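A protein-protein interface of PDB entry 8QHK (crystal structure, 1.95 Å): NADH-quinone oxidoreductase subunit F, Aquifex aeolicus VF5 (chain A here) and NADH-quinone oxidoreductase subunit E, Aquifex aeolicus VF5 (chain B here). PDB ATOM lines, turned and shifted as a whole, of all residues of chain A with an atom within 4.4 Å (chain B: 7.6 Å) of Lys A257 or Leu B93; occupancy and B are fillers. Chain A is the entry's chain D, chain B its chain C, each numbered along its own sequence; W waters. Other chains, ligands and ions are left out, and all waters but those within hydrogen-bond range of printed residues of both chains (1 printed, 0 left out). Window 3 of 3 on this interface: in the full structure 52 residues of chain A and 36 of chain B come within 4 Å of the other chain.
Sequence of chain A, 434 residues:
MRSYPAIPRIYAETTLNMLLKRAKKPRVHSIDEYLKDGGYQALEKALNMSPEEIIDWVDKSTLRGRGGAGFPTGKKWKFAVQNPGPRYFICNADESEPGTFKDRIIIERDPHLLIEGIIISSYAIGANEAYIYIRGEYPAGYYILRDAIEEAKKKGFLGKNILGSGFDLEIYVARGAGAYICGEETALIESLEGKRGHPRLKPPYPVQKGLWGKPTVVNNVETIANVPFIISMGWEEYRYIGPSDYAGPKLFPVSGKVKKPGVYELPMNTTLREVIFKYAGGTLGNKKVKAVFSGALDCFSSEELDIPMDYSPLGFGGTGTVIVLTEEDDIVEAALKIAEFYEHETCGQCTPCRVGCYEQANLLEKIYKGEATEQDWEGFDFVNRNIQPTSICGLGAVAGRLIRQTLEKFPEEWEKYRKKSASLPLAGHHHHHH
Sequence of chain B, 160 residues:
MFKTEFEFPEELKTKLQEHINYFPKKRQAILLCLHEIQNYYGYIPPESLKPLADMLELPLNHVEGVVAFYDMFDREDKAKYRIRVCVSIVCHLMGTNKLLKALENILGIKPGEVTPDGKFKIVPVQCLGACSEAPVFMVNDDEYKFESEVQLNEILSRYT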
ATOM      1  N   SER A 255      18.217  21.395   4.933  1.00  0.00           N
ATOM      2  CA  SER A 255      18.960  20.399   4.186  1.00  0.00           C
ATOM      3  C   SER A 255      18.210  19.065   4.161  1.00  0.00           C
ATOM      4  O   SER A 255      17.103  18.950   4.689  1.00  0.00           O
ATOM      5  CB  SER A 255      20.345  20.257   4.755  1.00  0.00           C
ATOM      6  OG  SER A 255      20.314  19.664   6.047  1.00  0.00           O
ATOM      7  N   GLY A 256      18.826  18.064   3.517  1.00  0.00           N
ATOM      8  CA  GLY A 256      18.225  16.755   3.334  1.00  0.00           C
ATOM      9  C   GLY A 256      17.338  16.736   2.094  1.00  0.00           C
ATOM     10  O   GLY A 256      17.681  17.324   1.063  1.00  0.00           O
ATOM     11  N   LYS A 257      16.160  16.128   2.227  1.00  0.00           N
ATOM     12  CA  LYS A 257      15.363  15.761   1.071  1.00  0.00           C
ATOM     13  C   LYS A 257      14.389  16.873   0.679  1.00  0.00           C
ATOM     14  O   LYS A 257      13.196  16.605   0.518  1.00  0.00           O
ATOM     15  CB  LYS A 257      14.623  14.457   1.378  1.00  0.00           C
ATOM     16  CG  LYS A 257      15.538  13.290   1.724  1.00  0.00           C
ATOM     17  CD  LYS A 257      16.447  12.892   0.574  1.00  0.00           C
ATOM     18  CE  LYS A 257      17.366  11.738   0.908  1.00  0.00           C
ATOM     19  NZ  LYS A 257      16.630  10.460   1.058  1.00  0.00           N
ATOM     20  N   VAL A 258      14.909  18.094   0.481  1.00  0.00           N
ATOM     21  CA  VAL A 258      14.123  19.200  -0.047  1.00  0.00           C
ATOM     22  C   VAL A 258      14.644  19.566  -1.436  1.00  0.00           C
ATOM     23  O   VAL A 258      15.782  19.252  -1.782  1.00  0.00           O
ATOM     24  CB  VAL A 258      14.132  20.425   0.889  1.00  0.00           C
ATOM     25  CG1 VAL A 258      13.510  20.099   2.235  1.00  0.00           C
ATOM     26  CG2 VAL A 258      15.522  21.032   1.074  1.00  0.00           C
ATOM     27  N   GLY A 282       9.322  22.079  -1.228  1.00  0.00           N
ATOM     28  CA  GLY A 282       8.804  20.744  -0.994  1.00  0.00           C
ATOM     29  C   GLY A 282       9.926  19.712  -0.992  1.00  0.00           C
ATOM     30  O   GLY A 282      11.103  20.065  -0.922  1.00  0.00           O
ATOM     31  N   THR A 283       9.530  18.441  -1.076  1.00  0.00           N
ATOM     32  CA  THR A 283      10.431  17.317  -0.903  1.00  0.00           C
ATOM     33  C   THR A 283      10.937  16.826  -2.255  1.00  0.00           C
ATOM     34  O   THR A 283      10.274  16.993  -3.281  1.00  0.00           O
ATOM     35  CB  THR A 283       9.743  16.177  -0.144  1.00  0.00           C
ATOM     36  OG1 THR A 283       8.548  15.821  -0.844  1.00  0.00           O
ATOM     37  CG2 THR A 283       9.412  16.538   1.287  1.00  0.00           C
ATOM     38  N   LEU A 284      12.124  16.208  -2.237  1.00  0.00           N
ATOM     39  CA  LEU A 284      12.639  15.523  -3.413  1.00  0.00           C
ATOM     40  C   LEU A 284      11.636  14.451  -3.826  1.00  0.00           C
ATOM     41  O   LEU A 284      11.162  13.691  -2.987  1.00  0.00           O
ATOM     42  CB  LEU A 284      13.996  14.888  -3.092  1.00  0.00           C
ATOM     43  CG  LEU A 284      15.192  15.834  -3.007  1.00  0.00           C
ATOM     44  CD1 LEU A 284      16.472  15.037  -2.801  1.00  0.00           C
ATOM     45  CD2 LEU A 284      15.312  16.711  -4.247  1.00  0.00           C
ATOM     46  N   VAL A 324      15.468  17.379   6.592  1.00  0.00           N
ATOM     47  CA  VAL A 324      14.267  16.666   6.188  1.00  0.00           C
ATOM     48  C   VAL A 324      14.622  15.237   5.768  1.00  0.00           C
ATOM     49  O   VAL A 324      15.493  15.019   4.923  1.00  0.00           O
ATOM     50  CB  VAL A 324      13.520  17.429   5.076  1.00  0.00           C
ATOM     51  CG1 VAL A 324      12.256  16.701   4.658  1.00  0.00           C
ATOM     52  CG2 VAL A 324      13.203  18.865   5.490  1.00  0.00           C
ATOM     53  N   LEU A 325      13.934  14.269   6.394  1.00  0.00           N
ATOM     54  CA  LEU A 325      13.936  12.876   5.977  1.00  0.00           C
ATOM     55  C   LEU A 325      12.576  12.546   5.373  1.00  0.00           C
ATOM     56  O   LEU A 325      11.550  12.987   5.889  1.00  0.00           O
ATOM     57  CB  LEU A 325      14.198  11.979   7.190  1.00  0.00           C
ATOM     58  CG  LEU A 325      15.627  11.984   7.734  1.00  0.00           C
ATOM     59  CD1 LEU A 325      15.932  13.260   8.488  1.00  0.00           C
ATOM     60  CD2 LEU A 325      15.863  10.779   8.633  1.00  0.00           C
ATOM     61  N   THR A 326      12.584  11.735   4.310  1.00  0.00           N
ATOM     62  CA  THR A 326      11.357  11.311   3.653  1.00  0.00           C
ATOM     63  C   THR A 326      11.128   9.817   3.882  1.00  0.00           C
ATOM     64  O   THR A 326      11.909   9.154   4.566  1.00  0.00           O
ATOM     65  CB  THR A 326      11.369  11.701   2.168  1.00  0.00           C
ATOM     66  OG1 THR A 326      12.561  11.193   1.567  1.00  0.00           O
ATOM     67  CG2 THR A 326      11.290  13.199   1.975  1.00  0.00           C
ATOM     68  N   GLU A 328      11.358   6.934   2.545  1.00  0.00           N
ATOM     69  CA  GLU A 328      12.272   5.833   2.278  1.00  0.00           C
ATOM     70  C   GLU A 328      13.429   5.811   3.279  1.00  0.00           C
ATOM     71  O   GLU A 328      14.104   4.790   3.393  1.00  0.00           O
ATOM     72  CB  GLU A 328      12.830   5.917   0.854  1.00  0.00           C
ATOM     73  CG  GLU A 328      13.926   6.956   0.672  1.00  0.00           C
ATOM     74  CD  GLU A 328      13.441   8.390   0.569  1.00  0.00           C
ATOM     75  OE1 GLU A 328      12.312   8.664   1.013  1.00  0.00           O
ATOM     76  OE2 GLU A 328      14.176   9.220  -0.002  1.00  0.00           O
ATOM     77  N   ASP A 329      13.634   6.912   4.019  1.00  0.00           N
ATOM     78  CA  ASP A 329      14.822   7.069   4.852  1.00  0.00           C
ATOM     79  C   ASP A 329      14.685   6.227   6.119  1.00  0.00           C
ATOM     80  O   ASP A 329      13.730   6.382   6.872  1.00  0.00           O
ATOM     81  CB  ASP A 329      15.099   8.540   5.166  1.00  0.00           C
ATOM     82  CG  ASP A 329      15.523   9.325   3.938  1.00  0.00           C
ATOM     83  OD1 ASP A 329      16.265   8.750   3.119  1.00  0.00           O
ATOM     84  OD2 ASP A 329      15.117  10.505   3.807  1.00  0.00           O
ATOM     85  N   VAL B  87      31.062  12.437   7.030  1.00  0.00           N
ATOM     86  CA  VAL B  87      30.359  11.178   7.215  1.00  0.00           C
ATOM     87  C   VAL B  87      29.162  11.356   8.151  1.00  0.00           C
ATOM     88  O   VAL B  87      28.621  10.368   8.633  1.00  0.00           O
ATOM     89  CB  VAL B  87      31.320  10.076   7.707  1.00  0.00           C
ATOM     90  CG1 VAL B  87      32.434   9.824   6.701  1.00  0.00           C
ATOM     91  CG2 VAL B  87      31.906  10.372   9.084  1.00  0.00           C
ATOM     92  N   SER B  88      28.720  12.596   8.385  1.00  0.00           N
ATOM     93  CA  SER B  88      27.592  12.848   9.275  1.00  0.00           C
ATOM     94  C   SER B  88      26.275  12.698   8.521  1.00  0.00           C
ATOM     95  O   SER B  88      26.269  12.411   7.326  1.00  0.00           O
ATOM     96  CB  SER B  88      27.698  14.202   9.929  1.00  0.00           C
ATOM     97  OG  SER B  88      28.763  14.221  10.851  1.00  0.00           O
ATOM     98  N   ILE B  89      25.172  12.923   9.245  1.00  0.00           N
ATOM     99  CA  ILE B  89      23.833  12.499   8.868  1.00  0.00           C
ATOM    100  C   ILE B  89      23.434  13.014   7.481  1.00  0.00           C
ATOM    101  O   ILE B  89      22.920  12.238   6.673  1.00  0.00           O
ATOM    102  CB  ILE B  89      22.808  12.893   9.959  1.00  0.00           C
ATOM    103  CG1 ILE B  89      21.371  12.544   9.552  1.00  0.00           C
ATOM    104  CG2 ILE B  89      22.906  14.358  10.350  1.00  0.00           C
ATOM    105  CD1 ILE B  89      21.116  11.079   9.453  1.00  0.00           C
ATOM    106  N   VAL B  90      23.618  14.309   7.188  1.00  0.00           N
ATOM    107  CA  VAL B  90      23.063  14.827   5.940  1.00  0.00           C
ATOM    108  C   VAL B  90      23.834  14.253   4.754  1.00  0.00           C
ATOM    109  O   VAL B  90      23.235  13.686   3.840  1.00  0.00           O
ATOM    110  CB  VAL B  90      22.976  16.360   5.869  1.00  0.00           C
ATOM    111  CG1 VAL B  90      22.197  16.784   4.629  1.00  0.00           C
ATOM    112  CG2 VAL B  90      22.345  16.950   7.118  1.00  0.00           C
ATOM    113  N   CYS B  91      25.162  14.349   4.791  1.00  0.00           N
ATOM    114  CA  CYS B  91      25.988  13.815   3.717  1.00  0.00           C
ATOM    115  C   CYS B  91      25.781  12.313   3.552  1.00  0.00           C
ATOM    116  O   CYS B  91      25.850  11.807   2.429  1.00  0.00           O
ATOM    117  CB  CYS B  91      27.452  14.144   3.948  1.00  0.00           C
ATOM    118  SG  CYS B  91      27.763  15.919   3.787  1.00  0.00           S
ATOM    119  N   HIS B  92      25.531  11.610   4.664  1.00  0.00           N
ATOM    120  CA  HIS B  92      25.242  10.185   4.603  1.00  0.00           C
ATOM    121  C   HIS B  92      23.970   9.940   3.791  1.00  0.00           C
ATOM    122  O   HIS B  92      23.965   9.099   2.901  1.00  0.00           O
ATOM    123  CB  HIS B  92      25.111   9.565   5.999  1.00  0.00           C
ATOM    124  CG  HIS B  92      24.745   8.122   5.898  1.00  0.00           C
ATOM    125  ND1 HIS B  92      25.636   7.163   5.461  1.00  0.00           N
ATOM    126  CD2 HIS B  92      23.587   7.491   6.117  1.00  0.00           C
ATOM    127  CE1 HIS B  92      25.027   5.984   5.443  1.00  0.00           C
ATOM    128  NE2 HIS B  92      23.780   6.160   5.832  1.00  0.00           N
ATOM    129  N   LEU B  93      22.900  10.666   4.136  1.00  0.00           N
ATOM    130  CA  LEU B  93      21.609  10.586   3.467  1.00  0.00           C
ATOM    131  C   LEU B  93      21.717  10.915   1.979  1.00  0.00           C
ATOM    132  O   LEU B  93      20.912  10.423   1.196  1.00  0.00           O
ATOM    133  CB  LEU B  93      20.646  11.582   4.127  1.00  0.00           C
ATOM    134  CG  LEU B  93      19.629  11.013   5.110  1.00  0.00           C
ATOM    135  CD1 LEU B  93      20.255   9.997   6.056  1.00  0.00           C
ATOM    136  CD2 LEU B  93      18.990  12.148   5.896  1.00  0.00           C
ATOM    137  N   MET B  94      22.653  11.796   1.605  1.00  0.00           N
ATOM    138  CA  MET B  94      22.667  12.369   0.266  1.00  0.00           C
ATOM    139  C   MET B  94      23.781  11.761  -0.585  1.00  0.00           C
ATOM    140  O   MET B  94      23.851  12.064  -1.769  1.00  0.00           O
ATOM    141  CB  MET B  94      22.844  13.890   0.318  1.00  0.00           C
ATOM    142  CG  MET B  94      21.761  14.601   1.129  1.00  0.00           C
ATOM    143  SD  MET B  94      20.066  14.229   0.605  1.00  0.00           S
ATOM    144  CE  MET B  94      20.148  14.685  -1.125  1.00  0.00           C
ATOM    145  N   GLY B  95      24.664  10.951   0.014  1.00  0.00           N
ATOM    146  CA  GLY B  95      25.490  10.045  -0.766  1.00  0.00           C
ATOM    147  C   GLY B  95      26.990  10.091  -0.468  1.00  0.00           C
ATOM    148  O   GLY B  95      27.790   9.965  -1.395  1.00  0.00           O
ATOM    149  N   THR B  96      27.367  10.174   0.821  1.00  0.00           N
ATOM    150  CA  THR B  96      28.751   9.973   1.249  1.00  0.00           C
ATOM    151  C   THR B  96      29.359   8.732   0.586  1.00  0.00           C
ATOM    152  O   THR B  96      30.509   8.764   0.148  1.00  0.00           O
ATOM    153  CB  THR B  96      28.861   9.838   2.777  1.00  0.00           C
ATOM    154  OG1 THR B  96      28.424  11.054   3.389  1.00  0.00           O
ATOM    155  CG2 THR B  96      30.263   9.512   3.251  1.00  0.00           C
ATOM    156  N   ASN B  97      28.594   7.633   0.517  1.00  0.00           N
ATOM    157  CA  ASN B  97      29.128   6.354   0.067  1.00  0.00           C
ATOM    158  C   ASN B  97      29.493   6.416  -1.416  1.00  0.00           C
ATOM    159  O   ASN B  97      30.478   5.810  -1.835  1.00  0.00           O
ATOM    160  CB  ASN B  97      28.174   5.199   0.390  1.00  0.00           C
ATOM    161  CG  ASN B  97      28.060   4.920   1.881  1.00  0.00           C
ATOM    162  OD1 ASN B  97      27.065   4.357   2.333  1.00  0.00           O
ATOM    163  ND2 ASN B  97      29.051   5.328   2.661  1.00  0.00           N
ATOM    164  N   ALA B 134      25.478  18.687   0.405  1.00  0.00           N
ATOM    165  CA  ALA B 134      25.847  17.298   0.628  1.00  0.00           C
ATOM    166  C   ALA B 134      25.818  16.528  -0.688  1.00  0.00           C
ATOM    167  O   ALA B 134      24.994  16.818  -1.561  1.00  0.00           O
ATOM    168  CB  ALA B 134      24.893  16.670   1.613  1.00  0.00           C
ATOM    169  N   PRO B 135      26.723  15.541  -0.889  1.00  0.00           N
ATOM    170  CA  PRO B 135      27.811  15.250   0.048  1.00  0.00           C
ATOM    171  C   PRO B 135      29.036  16.148  -0.118  1.00  0.00           C
ATOM    172  O   PRO B 135      29.468  16.414  -1.235  1.00  0.00           O
ATOM    173  CB  PRO B 135      28.169  13.796  -0.284  1.00  0.00           C
ATOM    174  CG  PRO B 135      27.810  13.626  -1.734  1.00  0.00           C
ATOM    175  CD  PRO B 135      26.699  14.610  -2.025  1.00  0.00           C
HETATM  176  O   HOH W   1      19.135   8.720   1.136  1.00  0.00           O
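N of Val A324 lies within hydrogen-bond range of O of Ser A255, 3.0 Å away.
The backbone carbonyl oxygen (O) of Lys A257 lies within hydrogen-bond range of the backbone NH (N) of Leu A284.
The backbone carbonyl oxygen (O) of Val A324 is in hydrogen-bond range of the backbone NH (N) of Lys A257 (3.0 Å).
NZ of Lys A257 is in salt-bridge range of OE2 of Glu A328, 2.9 Å away.
The side-chain amino group (NZ) of Lys A257 is in salt-bridge range of the side-chain carboxylate (OD1) of Asp A329, at 2.7 Å.
Among the printed residues, merely in contact across the chains: Ser A255 with Val B90 (3.6 Å), Lys A257 with Met B94 (3.7 Å), Gly A256 with Val B90 (3.8 Å), Lys A257 with Leu B93 (3.8 Å), Leu A325 with Leu B93 (3.8 Å) and Gly A256 with Met B94 (3.9 Å).
Leu B93 touches two residues of chain A.
Printed residues of chain B within 4 Å of Leu A325: Leu B93 (3.8 Å).
Printed residues of chain A within 4 Å of Met B94: Gly A256 (3.9 Å) and Lys A257 (3.7 Å).
Of the printed residues of chain A, Val B90 touches Ser A255 and Gly A256.
Of the printed residues of chain B, Ser A255 touches Val B90.
The nearest printed residue of chain A that does not touch Leu B93 is Asp A329 (4.5 Å).
The nearest printed residue of chain A that does not touch Met B94 is Leu A284 (4.1 Å).
Of the 12 printed residues of chain A, 4 touch a printed residue of chain B.
Hydrophobic or aromatic side chains of chain B within 4 Å of the printed part of chain A: Val B90, Leu B93 and Met B94.
Along chain B the printed residues that touch a printed residue of chain A span positions 90 to 94.
Among the printed residues, 6 pairs touch across the chains.
Water W1 lies within hydrogen-bond range of the backbone carbonyl oxygen of Leu B93 (2.5 Å), the side-chain amino group of Lys A257 (3.1 Å) and the side-chain carboxylate of Asp A329 (3.5 Å).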
